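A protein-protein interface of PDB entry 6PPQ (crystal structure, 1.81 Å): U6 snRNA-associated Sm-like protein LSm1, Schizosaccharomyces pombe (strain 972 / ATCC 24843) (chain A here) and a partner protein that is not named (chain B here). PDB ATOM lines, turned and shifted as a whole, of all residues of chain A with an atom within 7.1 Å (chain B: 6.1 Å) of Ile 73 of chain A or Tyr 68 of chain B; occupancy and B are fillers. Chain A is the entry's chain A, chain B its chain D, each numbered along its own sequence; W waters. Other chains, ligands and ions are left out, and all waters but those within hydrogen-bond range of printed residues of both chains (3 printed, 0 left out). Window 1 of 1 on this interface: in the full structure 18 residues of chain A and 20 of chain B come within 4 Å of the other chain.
Among the printed residues, pairs that only touch across the chains: Leu 30 of chain A with Tyr 68 of chain B (3.99 Å), Lys 34 of chain A with Tyr 68 of chain B (3.7 Å), Asp 44 of chain A with Leu 4 of chain B (3.99 Å), Asn 48 of chain A with Pro 3 of chain B (3.8 Å), Asn 48 of chain A with Met 36 of chain B (3.8 Å), Met 50 of chain A with Leu 6 of chain B (3.6 Å), Val 71 of chain A with Arg 70 of chain B (3.3 Å), Tyr 72 of chain A with Tyr 68 of chain B (3.7 Å), Tyr 72 of chain A with Leu 69 of chain B (3.3 Å), Tyr 72 of chain A with Arg 70 of chain B (3.6 Å), Ile 73 of chain A with Pro 3 of chain B (3.4 Å), Ile 73 of chain A with Leu 6 of chain B (3.97 Å), Ile 73 of chain A with Leu 7 of chain B (3.97 Å), Ile 73 of chain A with Tyr 68 of chain B (3.4 Å), Arg 75 of chain A with Met 36 of chain B (3.4 Å) and Arg 75 of chain A with Ile 66 of chain B (3.4 Å).
The backbone NH (N) of Ile 73 of chain A is in hydrogen-bond range of the backbone carbonyl oxygen (O) of Leu 69 of chain B, 2.9 Å away.
The guanidinium group (NE) of Arg 70 of chain B lies within hydrogen-bond range of the backbone carbonyl oxygen (O) of Arg 69 of chain A (2.9 Å).
O of Lys 67 of chain B lies within hydrogen-bond range of ND2 of Asn 78 of chain A (3.2 Å).
The side-chain carboxylate (OD2) of Asp 32 of chain A is in salt-bridge range of the side-chain amino group (NZ) of Lys 67 of chain B (2.6 Å).
OE1 of Glu 18 of chain B lies within salt-bridge range of NZ of Lys 34 of chain A (3.5 Å).
O of Lys 67 of chain B is in hydrogen-bond range of N of Arg 75 of chain A (3.2 Å).
O of Ile 66 of chain B sits at hydrogen-bond distance from ND2 of Asn 78 of chain A (3.0 Å).
N of Ile 71 of chain B lies within hydrogen-bond range of O of Val 71 of chain A, at 3.1 Å.
Of the 18 printed residues of chain A, 12 touch a printed residue of chain B.
Hydrophobic or aromatic side chains of chain A that line the printed part of chain B: Leu 30, Met 50, Val 71, Tyr 72 and Ile 73.
Of the 17 printed residues of chain B, 12 touch a printed residue of chain A.
Among the printed residues, 24 pairs touch across the chains.
Glu 56 of chain A touches none of the printed residues of chain B.
Ile 73 of chain A touches just these residues of chain B: Pro 3 (3.4 Å), Leu 6 (3.97 Å), Leu 7 (3.97 Å), Tyr 68 (3.4 Å) and Leu 69 (2.9 Å).
Of the printed residues of chain B, Asn 78 of chain A touches Ile 66 and Lys 67.
Of the printed residues of chain A, Leu 7 of chain B touches Ile 73.
Leu 16 of chain B touches none of the printed residues of chain A.
Of the printed residues of chain A, Tyr 68 of chain B touches Leu 30, Lys 34, Tyr 72 and Ile 73.
Of the printed residues of chain A, Ile 71 of chain B touches Val 71.
The nearest residue of chain B that does not touch Ile 73 of chain A is Lys 67 of chain B (4.8 Å).
The nearest printed residue of chain A that does not touch Tyr 68 of chain B is Val 74 of chain A (4.04 Å).
The nearest printed residue of chain B that does not touch Asp 32 of chain A is Glu 18 of chain B (4.2 Å).
The guanidinium group (NH1) of Arg 69 of chain A lies within salt-bridge range of the side-chain carboxylate (OE2) of Glu 56 of chain A (2.9 Å).
O of Leu 16 of chain B sits at hydrogen-bond distance from N of Arg 70 of chain B (2.8 Å).
N of Tyr 72 of chain A lies within hydrogen-bond range of O of Leu 51 of chain A.
The backbone carbonyl oxygen of Arg 75 of chain A sits at hydrogen-bond distance from the side-chain amide nitrogen of Asn 78 of chain A, 3.3 Å away.
The side-chain amino group of Lys 67 of chain B lies within salt-bridge range of the side-chain carboxylate of Glu 18 of chain B (2.8 Å).
Water W2 lies within hydrogen-bond range of the side-chain hydroxyl (OH) of Tyr 72 of chain A, the side-chain hydroxyl (OH) of Tyr 68 of chain B and the side-chain carboxylate (OE2) of Glu 56 of chain A.
Water W3 lies within hydrogen-bond range of NH2 of Arg 69 of chain A (2.6 Å) and NH2 of Arg 70 of chain B (3.0 Å).
Water W1 bridges the side-chain carboxylate (OD2) of Asp 44 of chain A (2.7 Å) and the backbone NH (N) of Leu 4 of chain B (2.9 Å).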
ATOM      1  N   LEU A  30      -3.331  21.099  11.114  1.00  0.00           N
ATOM      2  CA  LEU A  30      -4.484  20.452  11.726  1.00  0.00           C
ATOM      3  C   LEU A  30      -4.070  19.648  12.944  1.00  0.00           C
ATOM      4  O   LEU A  30      -2.906  19.274  13.112  1.00  0.00           O
ATOM      5  CB  LEU A  30      -5.184  19.513  10.738  1.00  0.00           C
ATOM      6  CG  LEU A  30      -5.616  20.131   9.403  1.00  0.00           C
ATOM      7  CD1 LEU A  30      -6.413  19.093   8.611  1.00  0.00           C
ATOM      8  CD2 LEU A  30      -6.462  21.356   9.692  1.00  0.00           C
ATOM      9  N   ASP A  32      -4.567  16.587  13.668  1.00  0.00           N
ATOM     10  CA  ASP A  32      -3.990  15.286  13.353  1.00  0.00           C
ATOM     11  C   ASP A  32      -2.591  15.392  12.756  1.00  0.00           C
ATOM     12  O   ASP A  32      -2.015  14.372  12.377  1.00  0.00           O
ATOM     13  CB  ASP A  32      -4.912  14.512  12.398  1.00  0.00           C
ATOM     14  CG  ASP A  32      -4.923  15.089  10.979  1.00  0.00           C
ATOM     15  OD1 ASP A  32      -4.412  16.209  10.762  1.00  0.00           O
ATOM     16  OD2 ASP A  32      -5.460  14.416  10.077  1.00  0.00           O
ATOM     17  N   LYS A  34      -1.714  17.039   9.905  1.00  0.00           N
ATOM     18  CA  LYS A  34      -1.643  17.302   8.467  1.00  0.00           C
ATOM     19  C   LYS A  34      -1.257  18.749   8.198  1.00  0.00           C
ATOM     20  O   LYS A  34      -1.609  19.657   8.955  1.00  0.00           O
ATOM     21  CB  LYS A  34      -2.984  17.023   7.784  1.00  0.00           C
ATOM     22  CG  LYS A  34      -3.333  15.557   7.592  1.00  0.00           C
ATOM     23  CD  LYS A  34      -4.575  15.420   6.704  1.00  0.00           C
ATOM     24  CE  LYS A  34      -4.814  13.970   6.310  1.00  0.00           C
ATOM     25  NZ  LYS A  34      -4.828  13.066   7.493  1.00  0.00           N
ATOM     26  N   LEU A  36      -1.705  21.549   5.230  1.00  0.00           N
ATOM     27  CA  LEU A  36      -2.396  21.934   4.004  1.00  0.00           C
ATOM     28  C   LEU A  36      -1.871  23.285   3.565  1.00  0.00           C
ATOM     29  O   LEU A  36      -1.752  24.192   4.385  1.00  0.00           O
ATOM     30  CB  LEU A  36      -3.909  22.013   4.227  1.00  0.00           C
ATOM     31  CG  LEU A  36      -4.586  20.764   4.825  1.00  0.00           C
ATOM     32  CD1 LEU A  36      -6.083  20.986   4.973  1.00  0.00           C
ATOM     33  CD2 LEU A  36      -4.312  19.570   3.928  1.00  0.00           C
ATOM     34  N   ASP A  44     -15.228  31.564   8.991  1.00  0.00           N
ATOM     35  CA  ASP A  44     -16.343  32.080   9.775  1.00  0.00           C
ATOM     36  C   ASP A  44     -15.986  32.199  11.252  1.00  0.00           C
ATOM     37  O   ASP A  44     -14.813  32.107  11.634  1.00  0.00           O
ATOM     38  CB  ASP A  44     -17.598  31.212   9.587  1.00  0.00           C
ATOM     39  CG  ASP A  44     -17.375  29.755   9.985  1.00  0.00           C
ATOM     40  OD1 ASP A  44     -16.477  29.505  10.808  1.00  0.00           O
ATOM     41  OD2 ASP A  44     -18.088  28.867   9.458  1.00  0.00           O
ATOM     42  N   ASN A  48     -13.900  27.868  10.949  1.00  0.00           N
ATOM     43  CA  ASN A  48     -14.047  27.045   9.755  1.00  0.00           C
ATOM     44  C   ASN A  48     -13.342  27.769   8.623  1.00  0.00           C
ATOM     45  O   ASN A  48     -13.418  28.993   8.536  1.00  0.00           O
ATOM     46  CB  ASN A  48     -15.511  26.862   9.347  1.00  0.00           C
ATOM     47  CG  ASN A  48     -16.311  26.069  10.330  1.00  0.00           C
ATOM     48  OD1 ASN A  48     -15.808  25.140  10.954  1.00  0.00           O
ATOM     49  ND2 ASN A  48     -17.588  26.424  10.462  1.00  0.00           N
ATOM     50  N   LEU A  49     -12.656  27.025   7.762  1.00  0.00           N
ATOM     51  CA  LEU A  49     -11.868  27.639   6.699  1.00  0.00           C
ATOM     52  C   LEU A  49     -12.275  27.076   5.350  1.00  0.00           C
ATOM     53  O   LEU A  49     -12.574  25.895   5.225  1.00  0.00           O
ATOM     54  CB  LEU A  49     -10.370  27.396   6.898  1.00  0.00           C
ATOM     55  CG  LEU A  49      -9.733  27.731   8.238  1.00  0.00           C
ATOM     56  CD1 LEU A  49      -8.267  27.296   8.223  1.00  0.00           C
ATOM     57  CD2 LEU A  49      -9.859  29.218   8.550  1.00  0.00           C
ATOM     58  N   MET A  50     -12.228  27.908   4.314  1.00  0.00           N
ATOM     59  CA  MET A  50     -12.379  27.412   2.957  1.00  0.00           C
ATOM     60  C   MET A  50     -11.127  27.790   2.183  1.00  0.00           C
ATOM     61  O   MET A  50     -10.780  28.983   2.113  1.00  0.00           O
ATOM     62  CB  MET A  50     -13.631  27.971   2.276  1.00  0.00           C
ATOM     63  CG  MET A  50     -14.024  27.160   1.063  1.00  0.00           C
ATOM     64  SD  MET A  50     -13.358  27.940  -0.413  1.00  0.00           S
ATOM     65  CE  MET A  50     -14.536  29.293  -0.527  1.00  0.00           C
ATOM     66  N   LEU A  51     -10.474  26.761   1.611  1.00  0.00           N
ATOM     67  CA  LEU A  51      -9.189  26.842   0.918  1.00  0.00           C
ATOM     68  C   LEU A  51      -9.324  26.357  -0.519  1.00  0.00           C
ATOM     69  O   LEU A  51      -9.939  25.316  -0.776  1.00  0.00           O
ATOM     70  CB  LEU A  51      -8.125  25.975   1.608  1.00  0.00           C
ATOM     71  CG  LEU A  51      -7.903  26.165   3.106  1.00  0.00           C
ATOM     72  CD1 LEU A  51      -7.103  24.993   3.678  1.00  0.00           C
ATOM     73  CD2 LEU A  51      -7.177  27.472   3.319  1.00  0.00           C
ATOM     74  N   GLU A  56      -1.789  18.968  -0.058  1.00  0.00           N
ATOM     75  CA  GLU A  56      -1.388  18.376   1.208  1.00  0.00           C
ATOM     76  C   GLU A  56       0.098  18.068   1.116  1.00  0.00           C
ATOM     77  O   GLU A  56       0.534  17.404   0.169  1.00  0.00           O
ATOM     78  CB  GLU A  56      -2.173  17.096   1.503  1.00  0.00           C
ATOM     79  CG  GLU A  56      -1.692  16.397   2.786  1.00  0.00           C
ATOM     80  CD  GLU A  56      -2.568  15.213   3.172  1.00  0.00           C
ATOM     81  OE1 GLU A  56      -2.233  14.521   4.154  1.00  0.00           O
ATOM     82  OE2 GLU A  56      -3.587  14.973   2.487  1.00  0.00           O
ATOM     83  N   ARG A  69      -5.014  18.492  -3.935  1.00  0.00           N
ATOM     84  CA  ARG A  69      -6.202  18.175  -3.151  1.00  0.00           C
ATOM     85  C   ARG A  69      -7.435  18.996  -3.495  1.00  0.00           C
ATOM     86  O   ARG A  69      -8.537  18.606  -3.088  1.00  0.00           O
ATOM     87  CB  ARG A  69      -5.920  18.352  -1.656  1.00  0.00           C
ATOM     88  CG  ARG A  69      -4.967  17.327  -1.066  1.00  0.00           C
ATOM     89  CD  ARG A  69      -5.515  15.920  -1.238  1.00  0.00           C
ATOM     90  NE  ARG A  69      -4.901  15.011  -0.284  1.00  0.00           N
ATOM     91  CZ  ARG A  69      -4.932  13.687  -0.375  1.00  0.00           C
ATOM     92  NH1 ARG A  69      -4.355  12.946   0.567  1.00  0.00           N
ATOM     93  NH2 ARG A  69      -5.548  13.102  -1.385  1.00  0.00           N
ATOM     94  N   VAL A  71     -10.291  21.837  -3.257  1.00  0.00           N
ATOM     95  CA  VAL A  71     -10.941  22.772  -2.343  1.00  0.00           C
ATOM     96  C   VAL A  71     -11.224  22.039  -1.043  1.00  0.00           C
ATOM     97  O   VAL A  71     -11.733  20.911  -1.065  1.00  0.00           O
ATOM     98  CB  VAL A  71     -12.245  23.322  -2.947  1.00  0.00           C
ATOM     99  CG1 VAL A  71     -13.029  24.113  -1.904  1.00  0.00           C
ATOM    100  CG2 VAL A  71     -11.956  24.181  -4.185  1.00  0.00           C
ATOM    101  N   TYR A  72     -10.903  22.672   0.078  1.00  0.00           N
ATOM    102  CA  TYR A  72     -11.249  22.153   1.401  1.00  0.00           C
ATOM    103  C   TYR A  72     -12.210  23.084   2.118  1.00  0.00           C
ATOM    104  O   TYR A  72     -12.090  24.312   2.029  1.00  0.00           O
ATOM    105  CB  TYR A  72     -10.037  22.040   2.334  1.00  0.00           C
ATOM    106  CG  TYR A  72      -9.103  20.883   2.114  1.00  0.00           C
ATOM    107  CD1 TYR A  72      -8.098  20.955   1.166  1.00  0.00           C
ATOM    108  CD2 TYR A  72      -9.178  19.748   2.908  1.00  0.00           C
ATOM    109  CE1 TYR A  72      -7.211  19.915   0.988  1.00  0.00           C
ATOM    110  CE2 TYR A  72      -8.304  18.702   2.736  1.00  0.00           C
ATOM    111  CZ  TYR A  72      -7.319  18.786   1.778  1.00  0.00           C
ATOM    112  OH  TYR A  72      -6.445  17.734   1.608  1.00  0.00           O
ATOM    113  N   ILE A  73     -13.093  22.490   2.921  1.00  0.00           N
ATOM    114  CA  ILE A  73     -13.734  23.187   4.024  1.00  0.00           C
ATOM    115  C   ILE A  73     -13.223  22.504   5.288  1.00  0.00           C
ATOM    116  O   ILE A  73     -13.548  21.339   5.534  1.00  0.00           O
ATOM    117  CB  ILE A  73     -15.265  23.137   3.949  1.00  0.00           C
ATOM    118  CG1 ILE A  73     -15.775  23.852   2.696  1.00  0.00           C
ATOM    119  CG2 ILE A  73     -15.872  23.754   5.208  1.00  0.00           C
ATOM    120  CD1 ILE A  73     -17.275  23.730   2.523  1.00  0.00           C
ATOM    121  N   VAL A  74     -12.395  23.201   6.052  1.00  0.00           N
ATOM    122  CA  VAL A  74     -11.833  22.650   7.282  1.00  0.00           C
ATOM    123  C   VAL A  74     -12.699  23.079   8.452  1.00  0.00           C
ATOM    124  O   VAL A  74     -12.980  24.273   8.632  1.00  0.00           O
ATOM    125  CB  VAL A  74     -10.378  23.102   7.477  1.00  0.00           C
ATOM    126  CG1 VAL A  74      -9.769  22.422   8.715  1.00  0.00           C
ATOM    127  CG2 VAL A  74      -9.563  22.794   6.218  1.00  0.00           C
ATOM    128  N   ARG A  75     -13.123  22.111   9.262  1.00  0.00           N
ATOM    129  CA  ARG A  75     -13.924  22.451  10.421  1.00  0.00           C
ATOM    130  C   ARG A  75     -13.015  23.065  11.482  1.00  0.00           C
ATOM    131  O   ARG A  75     -11.966  22.497  11.817  1.00  0.00           O
ATOM    132  CB  ARG A  75     -14.656  21.217  10.961  1.00  0.00           C
ATOM    133  CG  ARG A  75     -15.544  21.522  12.150  1.00  0.00           C
ATOM    134  CD  ARG A  75     -16.310  20.271  12.595  1.00  0.00           C
ATOM    135  NE  ARG A  75     -16.937  20.454  13.902  1.00  0.00           N
ATOM    136  CZ  ARG A  75     -18.167  20.920  14.080  1.00  0.00           C
ATOM    137  NH1 ARG A  75     -18.923  21.240  13.038  1.00  0.00           N
ATOM    138  NH2 ARG A  75     -18.658  21.045  15.297  1.00  0.00           N
ATOM    139  N   GLY A  76     -13.429  24.225  11.998  1.00  0.00           N
ATOM    140  CA  GLY A  76     -12.518  25.084  12.746  1.00  0.00           C
ATOM    141  C   GLY A  76     -11.856  24.402  13.930  1.00  0.00           C
ATOM    142  O   GLY A  76     -10.688  24.660  14.236  1.00  0.00           O
ATOM    143  N   ASN A  78     -10.549  21.681  14.253  1.00  0.00           N
ATOM    144  CA  ASN A  78      -9.379  20.887  13.926  1.00  0.00           C
ATOM    145  C   ASN A  78      -8.184  21.744  13.546  1.00  0.00           C
ATOM    146  O   ASN A  78      -7.106  21.203  13.299  1.00  0.00           O
ATOM    147  CB  ASN A  78      -9.712  19.919  12.785  1.00  0.00           C
ATOM    148  CG  ASN A  78     -10.883  19.023  13.135  1.00  0.00           C
ATOM    149  OD1 ASN A  78     -10.746  18.117  13.950  1.00  0.00           O
ATOM    150  ND2 ASN A  78     -12.053  19.322  12.588  1.00  0.00           N
ATOM    151  N   PRO B   3     -17.774  29.495   4.408  1.00  0.00           N
ATOM    152  CA  PRO B   3     -17.637  28.033   4.288  1.00  0.00           C
ATOM    153  C   PRO B   3     -18.954  27.276   4.275  1.00  0.00           C
ATOM    154  O   PRO B   3     -19.138  26.381   3.440  1.00  0.00           O
ATOM    155  CB  PRO B   3     -16.794  27.673   5.523  1.00  0.00           C
ATOM    156  CG  PRO B   3     -15.953  28.904   5.761  1.00  0.00           C
ATOM    157  CD  PRO B   3     -16.852  30.067   5.413  1.00  0.00           C
ATOM    158  N   LEU B   4     -19.880  27.605   5.178  1.00  0.00           N
ATOM    159  CA  LEU B   4     -21.143  26.872   5.241  1.00  0.00           C
ATOM    160  C   LEU B   4     -22.084  27.243   4.093  1.00  0.00           C
ATOM    161  O   LEU B   4     -22.910  26.419   3.680  1.00  0.00           O
ATOM    162  CB  LEU B   4     -21.809  27.112   6.597  1.00  0.00           C
ATOM    163  CG  LEU B   4     -20.967  26.609   7.776  1.00  0.00           C
ATOM    164  CD1 LEU B   4     -21.592  26.982   9.112  1.00  0.00           C
ATOM    165  CD2 LEU B   4     -20.774  25.115   7.678  1.00  0.00           C
ATOM    166  N   LEU B   6     -20.931  27.750   1.004  1.00  0.00           N
ATOM    167  CA  LEU B   6     -20.432  26.826  -0.006  1.00  0.00           C
ATOM    168  C   LEU B   6     -20.948  25.419   0.242  1.00  0.00           C
ATOM    169  O   LEU B   6     -21.381  24.731  -0.693  1.00  0.00           O
ATOM    170  CB  LEU B   6     -18.905  26.830  -0.022  1.00  0.00           C
ATOM    171  CG  LEU B   6     -18.293  25.806  -0.977  1.00  0.00           C
ATOM    172  CD1 LEU B   6     -18.697  26.105  -2.426  1.00  0.00           C
ATOM    173  CD2 LEU B   6     -16.781  25.781  -0.835  1.00  0.00           C
ATOM    174  N   LEU B   7     -20.907  24.970   1.500  1.00  0.00           N
ATOM    175  CA  LEU B   7     -21.412  23.636   1.811  1.00  0.00           C
ATOM    176  C   LEU B   7     -22.867  23.483   1.370  1.00  0.00           C
ATOM    177  O   LEU B   7     -23.236  22.484   0.740  1.00  0.00           O
ATOM    178  CB  LEU B   7     -21.258  23.354   3.308  1.00  0.00           C
ATOM    179  CG  LEU B   7     -21.666  21.943   3.713  1.00  0.00           C
ATOM    180  CD1 LEU B   7     -20.870  20.914   2.930  1.00  0.00           C
ATOM    181  CD2 LEU B   7     -21.482  21.740   5.216  1.00  0.00           C
ATOM    182  N   THR B  10     -23.210  22.985  -2.227  1.00  0.00           N
ATOM    183  CA  THR B  10     -22.710  21.698  -2.699  1.00  0.00           C
ATOM    184  C   THR B  10     -23.776  20.597  -2.699  1.00  0.00           C
ATOM    185  O   THR B  10     -23.518  19.503  -3.215  1.00  0.00           O
ATOM    186  CB  THR B  10     -21.488  21.311  -1.839  1.00  0.00           C
ATOM    187  OG1 THR B  10     -20.521  22.361  -1.931  1.00  0.00           O
ATOM    188  CG2 THR B  10     -20.814  20.025  -2.310  1.00  0.00           C
ATOM    189  N   LEU B  16     -16.228  14.667  -0.369  1.00  0.00           N
ATOM    190  CA  LEU B  16     -15.460  13.739   0.447  1.00  0.00           C
ATOM    191  C   LEU B  16     -15.469  14.284   1.863  1.00  0.00           C
ATOM    192  O   LEU B  16     -15.186  15.462   2.070  1.00  0.00           O
ATOM    193  CB  LEU B  16     -14.018  13.582  -0.079  1.00  0.00           C
ATOM    194  CG  LEU B  16     -13.048  12.725   0.753  1.00  0.00           C
ATOM    195  CD1 LEU B  16     -11.962  12.124  -0.115  1.00  0.00           C
ATOM    196  CD2 LEU B  16     -12.398  13.515   1.906  1.00  0.00           C
ATOM    197  N   VAL B  17     -15.791  13.439   2.836  1.00  0.00           N
ATOM    198  CA  VAL B  17     -15.820  13.824   4.241  1.00  0.00           C
ATOM    199  C   VAL B  17     -14.768  12.995   4.953  1.00  0.00           C
ATOM    200  O   VAL B  17     -14.783  11.768   4.851  1.00  0.00           O
ATOM    201  CB  VAL B  17     -17.206  13.573   4.872  1.00  0.00           C
ATOM    202  CG1 VAL B  17     -17.230  14.041   6.372  1.00  0.00           C
ATOM    203  CG2 VAL B  17     -18.292  14.231   4.060  1.00  0.00           C
ATOM    204  N   GLU B  18     -13.851  13.643   5.663  1.00  0.00           N
ATOM    205  CA  GLU B  18     -12.955  12.906   6.538  1.00  0.00           C
ATOM    206  C   GLU B  18     -13.377  13.165   7.975  1.00  0.00           C
ATOM    207  O   GLU B  18     -13.541  14.328   8.384  1.00  0.00           O
ATOM    208  CB  GLU B  18     -11.483  13.278   6.338  1.00  0.00           C
ATOM    209  CG  GLU B  18     -10.571  12.352   7.201  1.00  0.00           C
ATOM    210  CD  GLU B  18      -9.101  12.380   6.822  1.00  0.00           C
ATOM    211  OE1 GLU B  18      -8.252  12.264   7.727  1.00  0.00           O
ATOM    212  OE2 GLU B  18      -8.793  12.497   5.623  1.00  0.00           O
ATOM    213  N   LEU B  19     -13.545  12.074   8.732  1.00  0.00           N
ATOM    214  CA  LEU B  19     -13.930  12.160  10.133  1.00  0.00           C
ATOM    215  C   LEU B  19     -12.703  12.351  11.017  1.00  0.00           C
ATOM    216  O   LEU B  19     -11.562  12.143  10.599  1.00  0.00           O
ATOM    217  CB  LEU B  19     -14.699  10.902  10.549  1.00  0.00           C
ATOM    218  CG  LEU B  19     -15.992  10.602   9.794  1.00  0.00           C
ATOM    219  CD1 LEU B  19     -16.739   9.449  10.487  1.00  0.00           C
ATOM    220  CD2 LEU B  19     -16.864  11.855   9.678  1.00  0.00           C
ATOM    221  N   THR B  24     -12.983   8.024   5.862  1.00  0.00           N
ATOM    222  CA  THR B  24     -13.460   8.915   4.810  1.00  0.00           C
ATOM    223  C   THR B  24     -14.753   8.384   4.211  1.00  0.00           C
ATOM    224  O   THR B  24     -14.965   7.177   4.125  1.00  0.00           O
ATOM    225  CB  THR B  24     -12.435   9.101   3.677  1.00  0.00           C
ATOM    226  OG1 THR B  24     -12.194   7.844   3.048  1.00  0.00           O
ATOM    227  CG2 THR B  24     -11.124   9.658   4.209  1.00  0.00           C
ATOM    228  N   MET B  36     -23.224  21.597  10.694  1.00  0.00           N
ATOM    229  CA  MET B  36     -22.444  20.782   9.772  1.00  0.00           C
ATOM    230  C   MET B  36     -22.802  19.295   9.850  1.00  0.00           C
ATOM    231  O   MET B  36     -22.047  18.455   9.359  1.00  0.00           O
ATOM    232  CB  MET B  36     -20.937  20.978   9.975  1.00  0.00           C
ATOM    233  CG  MET B  36     -20.090  20.749   8.741  1.00  0.00           C
ATOM    234  SD  MET B  36     -18.348  21.048   9.121  1.00  0.00           S
ATOM    235  CE  MET B  36     -18.509  22.609   9.949  1.00  0.00           C
ATOM    236  N   ILE B  66     -16.576  15.710  12.304  1.00  0.00           N
ATOM    237  CA  ILE B  66     -15.948  15.975  11.006  1.00  0.00           C
ATOM    238  C   ILE B  66     -14.574  16.592  11.216  1.00  0.00           C
ATOM    239  O   ILE B  66     -14.394  17.476  12.061  1.00  0.00           O
ATOM    240  CB  ILE B  66     -16.845  16.890  10.150  1.00  0.00           C
ATOM    241  CG1 ILE B  66     -18.098  16.111   9.714  1.00  0.00           C
ATOM    242  CG2 ILE B  66     -16.072  17.437   8.902  1.00  0.00           C
ATOM    243  CD1 ILE B  66     -19.144  16.951   8.999  1.00  0.00           C
ATOM    244  N   LYS B  67     -13.595  16.120  10.439  1.00  0.00           N
ATOM    245  CA  LYS B  67     -12.301  16.779  10.339  1.00  0.00           C
ATOM    246  C   LYS B  67     -12.347  17.811   9.217  1.00  0.00           C
ATOM    247  O   LYS B  67     -12.203  19.014   9.455  1.00  0.00           O
ATOM    248  CB  LYS B  67     -11.189  15.750  10.080  1.00  0.00           C
ATOM    249  CG  LYS B  67      -9.763  16.322  10.138  1.00  0.00           C
ATOM    250  CD  LYS B  67      -8.702  15.272   9.756  1.00  0.00           C
ATOM    251  CE  LYS B  67      -8.768  14.021  10.640  1.00  0.00           C
ATOM    252  NZ  LYS B  67      -7.651  13.073  10.345  1.00  0.00           N
ATOM    253  N   TYR B  68     -12.588  17.353   7.996  1.00  0.00           N
ATOM    254  CA  TYR B  68     -12.721  18.315   6.905  1.00  0.00           C
ATOM    255  C   TYR B  68     -13.573  17.719   5.801  1.00  0.00           C
ATOM    256  O   TYR B  68     -13.894  16.534   5.804  1.00  0.00           O
ATOM    257  CB  TYR B  68     -11.347  18.755   6.340  1.00  0.00           C
ATOM    258  CG  TYR B  68     -10.469  17.596   5.873  1.00  0.00           C
ATOM    259  CD1 TYR B  68     -10.807  16.827   4.756  1.00  0.00           C
ATOM    260  CD2 TYR B  68      -9.298  17.290   6.531  1.00  0.00           C
ATOM    261  CE1 TYR B  68     -10.003  15.765   4.341  1.00  0.00           C
ATOM    262  CE2 TYR B  68      -8.491  16.238   6.119  1.00  0.00           C
ATOM    263  CZ  TYR B  68      -8.849  15.484   5.032  1.00  0.00           C
ATOM    264  OH  TYR B  68      -8.032  14.457   4.637  1.00  0.00           O
ATOM    265  N   LEU B  69     -13.918  18.575   4.837  1.00  0.00           N
ATOM    266  CA  LEU B  69     -14.624  18.193   3.627  1.00  0.00           C
ATOM    267  C   LEU B  69     -13.796  18.636   2.434  1.00  0.00           C
ATOM    268  O   LEU B  69     -13.129  19.668   2.488  1.00  0.00           O
ATOM    269  CB  LEU B  69     -16.000  18.866   3.535  1.00  0.00           C
ATOM    270  CG  LEU B  69     -16.811  18.813   4.834  1.00  0.00           C
ATOM    271  CD1 LEU B  69     -18.156  19.465   4.668  1.00  0.00           C
ATOM    272  CD2 LEU B  69     -16.998  17.372   5.203  1.00  0.00           C
ATOM    273  N   ARG B  70     -13.851  17.855   1.364  1.00  0.00           N
ATOM    274  CA  ARG B  70     -13.270  18.248   0.081  1.00  0.00           C
ATOM    275  C   ARG B  70     -14.368  18.289  -0.970  1.00  0.00           C
ATOM    276  O   ARG B  70     -15.250  17.418  -1.011  1.00  0.00           O
ATOM    277  CB  ARG B  70     -12.155  17.293  -0.353  1.00  0.00           C
ATOM    278  CG  ARG B  70     -10.881  17.462   0.475  1.00  0.00           C
ATOM    279  CD  ARG B  70      -9.825  16.413   0.137  1.00  0.00           C
ATOM    280  NE  ARG B  70      -9.458  16.487  -1.268  1.00  0.00           N
ATOM    281  CZ  ARG B  70      -9.088  15.443  -2.000  1.00  0.00           C
ATOM    282  NH1 ARG B  70      -9.028  14.233  -1.454  1.00  0.00           N
ATOM    283  NH2 ARG B  70      -8.782  15.611  -3.280  1.00  0.00           N
ATOM    284  N   ILE B  71     -14.320  19.318  -1.817  1.00  0.00           N
ATOM    285  CA  ILE B  71     -15.280  19.458  -2.901  1.00  0.00           C
ATOM    286  C   ILE B  71     -14.518  19.818  -4.167  1.00  0.00           C
ATOM    287  O   ILE B  71     -13.369  20.266  -4.121  1.00  0.00           O
ATOM    288  CB  ILE B  71     -16.374  20.506  -2.586  1.00  0.00           C
ATOM    289  CG1 ILE B  71     -15.805  21.910  -2.634  1.00  0.00           C
ATOM    290  CG2 ILE B  71     -16.992  20.266  -1.193  1.00  0.00           C
ATOM    291  CD1 ILE B  71     -16.859  22.949  -2.871  1.00  0.00           C
HETATM  292  O   HOH W   1     -19.635  29.554   7.341  1.00  0.00           O
HETATM  293  O   HOH W   2      -6.383  15.487   2.893  1.00  0.00           O
HETATM  294  O   HOH W   3      -6.346  13.883  -3.751  1.00  0.00           O
